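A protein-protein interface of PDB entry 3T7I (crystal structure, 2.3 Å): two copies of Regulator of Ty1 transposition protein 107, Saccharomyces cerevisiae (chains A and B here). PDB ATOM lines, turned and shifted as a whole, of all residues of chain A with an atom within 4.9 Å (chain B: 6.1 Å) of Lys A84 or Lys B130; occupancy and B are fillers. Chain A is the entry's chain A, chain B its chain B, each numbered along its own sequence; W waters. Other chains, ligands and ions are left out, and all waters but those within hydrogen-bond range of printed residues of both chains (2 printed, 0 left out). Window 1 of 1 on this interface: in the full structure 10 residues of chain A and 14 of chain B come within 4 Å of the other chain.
3 positions are printed for both chains.
Water W2 bridges the backbone carbonyl oxygen (O) of Lys B130 (2.9 Å) and the backbone carbonyl oxygen (O) of Tyr A21 (2.9 Å). Water W1 lies within hydrogen-bond range of NZ of Lys B130 (3.1 Å) and O of Leu A83 (3.3 Å).
The side-chain sulfur (SG) of Cys A62 lies close to the backbone carbonyl oxygen (O) of Phe A85. NZ of Lys A84 lies within salt-bridge range of OD2 of Asp A22 (3.98 Å). O of Tyr A21 is in hydrogen-bond range of NZ of Lys A84 (3.1 Å). The backbone NH (N) of Lys A84 sits at hydrogen-bond distance from the backbone carbonyl oxygen (O) of Asn A61. The backbone carbonyl oxygen (O) of Asn A61 is in hydrogen-bond range of the backbone NH (N) of Phe A85 (3.3 Å).
The side-chain amino group (NZ) of Lys B130 sits at hydrogen-bond distance from the backbone carbonyl oxygen (O) of Lys A84 (2.8 Å).
Of the 10 printed residues of chain B, 2 touch a printed residue of chain A. Hydrophobic or aromatic side chains of chain B that line the printed part of chain A: Pro B132. Of the 11 printed residues of chain A, 3 touch a printed residue of chain B. Hydrophobic or aromatic side chains of chain A within 4 Å of the printed part of chain B: Tyr A21 and Phe A85. Among the printed residues, no Asp or Glu carboxylate lies within 4 Å of a Lys or Arg side-chain nitrogen of the other chain.
Printed residues of chain B within 4 Å of Lys A84: Lys B130 (2.8 Å). Lys B130 touches just these residues of chain A: Lys A84 (2.8 Å) and Phe A85 (3.7 Å). Of the printed residues of chain A, Pro B132 touches Tyr A21 (3.6 Å). Of the printed residues of chain B, Phe A85 touches Lys B130. Of the printed residues of chain B, Tyr A21 touches Pro B132 (3.6 Å). Pro A82 touches none of the printed residues of chain B. Leu B131 touches none of the printed residues of chain A. The nearest printed residue of chain B that does not touch Phe A85 is Leu B131 (4.6 Å).
Among the printed residues, pairs that only touch across the chains: Tyr A21 with Pro B132 and Phe A85 with Lys B130.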
ATOM      1  N   TYR A  21       6.966 -18.193  -1.479  1.00  0.00           N
ATOM      2  CA  TYR A  21       7.853 -19.217  -2.042  1.00  0.00           C
ATOM      3  C   TYR A  21       9.289 -18.763  -2.263  1.00  0.00           C
ATOM      4  O   TYR A  21      10.167 -19.599  -2.437  1.00  0.00           O
ATOM      5  CB  TYR A  21       7.298 -19.780  -3.348  1.00  0.00           C
ATOM      6  CG  TYR A  21       6.028 -20.554  -3.166  1.00  0.00           C
ATOM      7  CD1 TYR A  21       6.050 -21.857  -2.684  1.00  0.00           C
ATOM      8  CD2 TYR A  21       4.798 -19.974  -3.458  1.00  0.00           C
ATOM      9  CE1 TYR A  21       4.880 -22.571  -2.508  1.00  0.00           C
ATOM     10  CE2 TYR A  21       3.624 -20.682  -3.284  1.00  0.00           C
ATOM     11  CZ  TYR A  21       3.672 -21.976  -2.805  1.00  0.00           C
ATOM     12  OH  TYR A  21       2.503 -22.674  -2.638  1.00  0.00           O
ATOM     13  N   ASP A  22       9.510 -17.452  -2.269  1.00  0.00           N
ATOM     14  CA  ASP A  22      10.825 -16.875  -2.495  1.00  0.00           C
ATOM     15  C   ASP A  22      11.531 -17.509  -3.705  1.00  0.00           C
ATOM     16  O   ASP A  22      12.625 -18.065  -3.585  1.00  0.00           O
ATOM     17  CB  ASP A  22      11.674 -17.016  -1.239  1.00  0.00           C
ATOM     18  CG  ASP A  22      13.008 -16.290  -1.342  1.00  0.00           C
ATOM     19  OD1 ASP A  22      13.099 -15.265  -2.060  1.00  0.00           O
ATOM     20  OD2 ASP A  22      13.973 -16.757  -0.695  1.00  0.00           O
ATOM     21  N   LEU A  23      10.897 -17.409  -4.870  1.00  0.00           N
ATOM     22  CA  LEU A  23      11.478 -17.924  -6.101  1.00  0.00           C
ATOM     23  C   LEU A  23      11.872 -16.776  -7.001  1.00  0.00           C
ATOM     24  O   LEU A  23      11.058 -15.911  -7.328  1.00  0.00           O
ATOM     25  CB  LEU A  23      10.525 -18.856  -6.855  1.00  0.00           C
ATOM     26  CG  LEU A  23       9.959 -20.060  -6.106  1.00  0.00           C
ATOM     27  CD1 LEU A  23       8.998 -20.847  -6.997  1.00  0.00           C
ATOM     28  CD2 LEU A  23      11.091 -20.946  -5.593  1.00  0.00           C
ATOM     29  N   ASN A  61      17.314 -18.503  -8.235  1.00  0.00           N
ATOM     30  CA  ASN A  61      17.384 -19.765  -7.516  1.00  0.00           C
ATOM     31  C   ASN A  61      16.441 -20.817  -8.078  1.00  0.00           C
ATOM     32  O   ASN A  61      16.266 -21.870  -7.468  1.00  0.00           O
ATOM     33  CB  ASN A  61      17.139 -19.545  -6.006  1.00  0.00           C
ATOM     34  CG  ASN A  61      15.728 -19.042  -5.692  1.00  0.00           C
ATOM     35  OD1 ASN A  61      14.854 -18.998  -6.563  1.00  0.00           O
ATOM     36  ND2 ASN A  61      15.507 -18.660  -4.441  1.00  0.00           N
ATOM     37  N   CYS A  62      15.857 -20.558  -9.251  1.00  0.00           N
ATOM     38  CA  CYS A  62      14.781 -21.411  -9.739  1.00  0.00           C
ATOM     39  C   CYS A  62      14.652 -21.416 -11.255  1.00  0.00           C
ATOM     40  O   CYS A  62      14.830 -20.408 -11.911  1.00  0.00           O
ATOM     41  CB  CYS A  62      13.444 -20.986  -9.094  1.00  0.00           C
ATOM     42  SG  CYS A  62      11.955 -21.949  -9.612  1.00  0.00           S
ATOM     43  N   PRO A  82      22.355 -21.271  -4.528  1.00  0.00           N
ATOM     44  CA  PRO A  82      22.238 -22.516  -5.287  1.00  0.00           C
ATOM     45  C   PRO A  82      21.026 -22.482  -6.221  1.00  0.00           C
ATOM     46  O   PRO A  82      20.290 -21.487  -6.274  1.00  0.00           O
ATOM     47  CB  PRO A  82      22.017 -23.556  -4.186  1.00  0.00           C
ATOM     48  CG  PRO A  82      21.201 -22.814  -3.159  1.00  0.00           C
ATOM     49  CD  PRO A  82      21.626 -21.340  -3.247  1.00  0.00           C
ATOM     50  N   LEU A  83      20.833 -23.564  -6.964  1.00  0.00           N
ATOM     51  CA  LEU A  83      19.556 -23.803  -7.624  1.00  0.00           C
ATOM     52  C   LEU A  83      18.664 -24.413  -6.544  1.00  0.00           C
ATOM     53  O   LEU A  83      18.955 -25.474  -6.039  1.00  0.00           O
ATOM     54  CB  LEU A  83      19.720 -24.757  -8.813  1.00  0.00           C
ATOM     55  CG  LEU A  83      18.463 -25.088  -9.639  1.00  0.00           C
ATOM     56  CD1 LEU A  83      17.772 -23.826 -10.148  1.00  0.00           C
ATOM     57  CD2 LEU A  83      18.769 -26.034 -10.810  1.00  0.00           C
ATOM     58  N   LYS A  84      17.608 -23.718  -6.157  1.00  0.00           N
ATOM     59  CA  LYS A  84      16.726 -24.220  -5.103  1.00  0.00           C
ATOM     60  C   LYS A  84      15.656 -25.171  -5.628  1.00  0.00           C
ATOM     61  O   LYS A  84      15.450 -26.246  -5.072  1.00  0.00           O
ATOM     62  CB  LYS A  84      16.093 -23.055  -4.354  1.00  0.00           C
ATOM     63  CG  LYS A  84      15.047 -23.457  -3.331  1.00  0.00           C
ATOM     64  CD  LYS A  84      14.703 -22.281  -2.426  1.00  0.00           C
ATOM     65  CE  LYS A  84      13.355 -21.666  -2.773  1.00  0.00           C
ATOM     66  NZ  LYS A  84      13.107 -20.432  -1.950  1.00  0.00           N
ATOM     67  N   PHE A  85      14.970 -24.769  -6.695  1.00  0.00           N
ATOM     68  CA  PHE A  85      13.959 -25.637  -7.316  1.00  0.00           C
ATOM     69  C   PHE A  85      14.092 -25.681  -8.832  1.00  0.00           C
ATOM     70  O   PHE A  85      14.398 -24.683  -9.472  1.00  0.00           O
ATOM     71  CB  PHE A  85      12.529 -25.205  -6.944  1.00  0.00           C
ATOM     72  CG  PHE A  85      12.197 -25.357  -5.472  1.00  0.00           C
ATOM     73  CD1 PHE A  85      12.193 -26.613  -4.873  1.00  0.00           C
ATOM     74  CD2 PHE A  85      11.887 -24.246  -4.698  1.00  0.00           C
ATOM     75  CE1 PHE A  85      11.899 -26.763  -3.501  1.00  0.00           C
ATOM     76  CE2 PHE A  85      11.585 -24.381  -3.329  1.00  0.00           C
ATOM     77  CZ  PHE A  85      11.588 -25.645  -2.737  1.00  0.00           C
ATOM     78  N   ALA A  86      13.867 -26.857  -9.397  1.00  0.00           N
ATOM     79  CA  ALA A  86      13.648 -26.997 -10.824  1.00  0.00           C
ATOM     80  C   ALA A  86      12.234 -27.531 -10.961  1.00  0.00           C
ATOM     81  O   ALA A  86      11.971 -28.670 -10.604  1.00  0.00           O
ATOM     82  CB  ALA A  86      14.651 -27.941 -11.423  1.00  0.00           C
ATOM     83  N   ILE A 126      21.283 -31.414  -8.171  1.00  0.00           N
ATOM     84  CA  ILE A 126      20.946 -30.044  -7.799  1.00  0.00           C
ATOM     85  C   ILE A 126      21.675 -29.565  -6.537  1.00  0.00           C
ATOM     86  O   ILE A 126      22.083 -28.407  -6.459  1.00  0.00           O
ATOM     87  CB  ILE A 126      19.431 -29.883  -7.619  1.00  0.00           C
ATOM     88  CG1 ILE A 126      18.735 -30.074  -8.966  1.00  0.00           C
ATOM     89  CG2 ILE A 126      19.096 -28.516  -7.045  1.00  0.00           C
ATOM     90  N   PHE B  80      16.082 -25.130  10.064  1.00  0.00           N
ATOM     91  CA  PHE B  80      16.900 -24.082   9.403  1.00  0.00           C
ATOM     92  C   PHE B  80      16.299 -23.690   8.035  1.00  0.00           C
ATOM     93  O   PHE B  80      15.556 -24.463   7.448  1.00  0.00           O
ATOM     94  CB  PHE B  80      18.357 -24.530   9.241  1.00  0.00           C
ATOM     95  CG  PHE B  80      19.109 -24.638  10.546  1.00  0.00           C
ATOM     96  CD1 PHE B  80      20.379 -25.185  10.587  1.00  0.00           C
ATOM     97  CD2 PHE B  80      18.544 -24.182  11.731  1.00  0.00           C
ATOM     98  CE1 PHE B  80      21.081 -25.301  11.802  1.00  0.00           C
ATOM     99  CE2 PHE B  80      19.229 -24.290  12.942  1.00  0.00           C
ATOM    100  CZ  PHE B  80      20.514 -24.855  12.968  1.00  0.00           C
ATOM    101  N   PRO B  82      17.401 -22.367   4.491  1.00  0.00           N
ATOM    102  CA  PRO B  82      17.204 -23.806   4.672  1.00  0.00           C
ATOM    103  C   PRO B  82      18.339 -24.469   5.461  1.00  0.00           C
ATOM    104  O   PRO B  82      19.303 -23.824   5.895  1.00  0.00           O
ATOM    105  CB  PRO B  82      17.246 -24.329   3.237  1.00  0.00           C
ATOM    106  CG  PRO B  82      18.304 -23.415   2.570  1.00  0.00           C
ATOM    107  CD  PRO B  82      18.194 -22.063   3.281  1.00  0.00           C
ATOM    108  N   LEU B  83      18.207 -25.779   5.632  1.00  0.00           N
ATOM    109  CA  LEU B  83      19.308 -26.617   6.041  1.00  0.00           C
ATOM    110  C   LEU B  83      20.073 -26.944   4.761  1.00  0.00           C
ATOM    111  O   LEU B  83      19.548 -27.579   3.865  1.00  0.00           O
ATOM    112  CB  LEU B  83      18.793 -27.909   6.707  1.00  0.00           C
ATOM    113  CG  LEU B  83      19.871 -28.861   7.230  1.00  0.00           C
ATOM    114  CD1 LEU B  83      20.818 -28.156   8.209  1.00  0.00           C
ATOM    115  CD2 LEU B  83      19.235 -30.087   7.898  1.00  0.00           C
ATOM    116  N   ILE B 126      16.061 -32.960   3.591  1.00  0.00           N
ATOM    117  CA  ILE B 126      16.720 -31.656   3.555  1.00  0.00           C
ATOM    118  C   ILE B 126      15.975 -30.645   2.677  1.00  0.00           C
ATOM    119  O   ILE B 126      15.844 -29.474   3.045  1.00  0.00           O
ATOM    120  CB  ILE B 126      18.192 -31.764   3.065  1.00  0.00           C
ATOM    121  CG1 ILE B 126      19.053 -32.450   4.111  1.00  0.00           C
ATOM    122  CG2 ILE B 126      18.775 -30.377   2.772  1.00  0.00           C
ATOM    123  CD1 ILE B 126      20.533 -32.393   3.810  1.00  0.00           C
ATOM    124  N   SER B 127      15.494 -31.075   1.516  1.00  0.00           N
ATOM    125  CA  SER B 127      14.832 -30.129   0.628  1.00  0.00           C
ATOM    126  C   SER B 127      13.507 -29.601   1.169  1.00  0.00           C
ATOM    127  O   SER B 127      13.031 -28.537   0.744  1.00  0.00           O
ATOM    128  CB  SER B 127      14.625 -30.734  -0.757  1.00  0.00           C
ATOM    129  OG  SER B 127      13.671 -31.783  -0.709  1.00  0.00           O
ATOM    130  N   LYS B 128      12.904 -30.327   2.109  1.00  0.00           N
ATOM    131  CA  LYS B 128      11.666 -29.847   2.710  1.00  0.00           C
ATOM    132  C   LYS B 128      11.915 -28.586   3.513  1.00  0.00           C
ATOM    133  O   LYS B 128      10.994 -27.834   3.789  1.00  0.00           O
ATOM    134  CB  LYS B 128      11.000 -30.928   3.569  1.00  0.00           C
ATOM    135  CG  LYS B 128      10.369 -32.055   2.730  1.00  0.00           C
ATOM    136  CD  LYS B 128       9.652 -33.050   3.631  1.00  0.00           C
ATOM    137  CE  LYS B 128       8.923 -34.099   2.797  1.00  0.00           C
ATOM    138  NZ  LYS B 128       9.820 -34.691   1.763  1.00  0.00           N
ATOM    139  N   THR B 129      13.171 -28.341   3.871  1.00  0.00           N
ATOM    140  CA  THR B 129      13.489 -27.130   4.626  1.00  0.00           C
ATOM    141  C   THR B 129      13.498 -25.897   3.724  1.00  0.00           C
ATOM    142  O   THR B 129      13.650 -24.795   4.216  1.00  0.00           O
ATOM    143  CB  THR B 129      14.846 -27.224   5.373  1.00  0.00           C
ATOM    144  OG1 THR B 129      15.918 -27.261   4.424  1.00  0.00           O
ATOM    145  CG2 THR B 129      14.892 -28.476   6.281  1.00  0.00           C
ATOM    146  N   LYS B 130      13.356 -26.100   2.411  1.00  0.00           N
ATOM    147  CA  LYS B 130      13.263 -25.006   1.445  1.00  0.00           C
ATOM    148  C   LYS B 130      11.804 -24.598   1.231  1.00  0.00           C
ATOM    149  O   LYS B 130      11.528 -23.607   0.556  1.00  0.00           O
ATOM    150  CB  LYS B 130      13.905 -25.383   0.088  1.00  0.00           C
ATOM    151  CG  LYS B 130      15.412 -25.611   0.160  1.00  0.00           C
ATOM    152  CD  LYS B 130      16.039 -25.905  -1.226  1.00  0.00           C
ATOM    153  CE  LYS B 130      15.975 -27.381  -1.577  1.00  0.00           C
ATOM    154  NZ  LYS B 130      16.564 -27.711  -2.917  1.00  0.00           N
ATOM    155  N   LEU B 131      10.878 -25.360   1.802  1.00  0.00           N
ATOM    156  CA  LEU B 131       9.445 -25.037   1.680  1.00  0.00           C
ATOM    157  C   LEU B 131       9.089 -23.730   2.385  1.00  0.00           C
ATOM    158  O   LEU B 131       9.804 -23.292   3.276  1.00  0.00           O
ATOM    159  CB  LEU B 131       8.572 -26.188   2.188  1.00  0.00           C
ATOM    160  CG  LEU B 131       8.666 -27.438   1.311  1.00  0.00           C
ATOM    161  CD1 LEU B 131       8.009 -28.624   1.998  1.00  0.00           C
ATOM    162  CD2 LEU B 131       8.031 -27.185  -0.054  1.00  0.00           C
ATOM    163  N   PRO B 132       7.988 -23.085   1.960  1.00  0.00           N
ATOM    164  CA  PRO B 132       7.528 -21.864   2.630  1.00  0.00           C
ATOM    165  C   PRO B 132       6.930 -22.104   4.041  1.00  0.00           C
ATOM    166  O   PRO B 132       6.773 -21.133   4.785  1.00  0.00           O
ATOM    167  CB  PRO B 132       6.456 -21.317   1.671  1.00  0.00           C
ATOM    168  CG  PRO B 132       5.982 -22.511   0.905  1.00  0.00           C
ATOM    169  CD  PRO B 132       7.193 -23.399   0.759  1.00  0.00           C
HETATM  170  O   HOH W   1      19.336 -26.296  -2.886  1.00  0.00           O
HETATM  171  O   HOH W   2       9.670 -22.179  -1.165  1.00  0.00           O
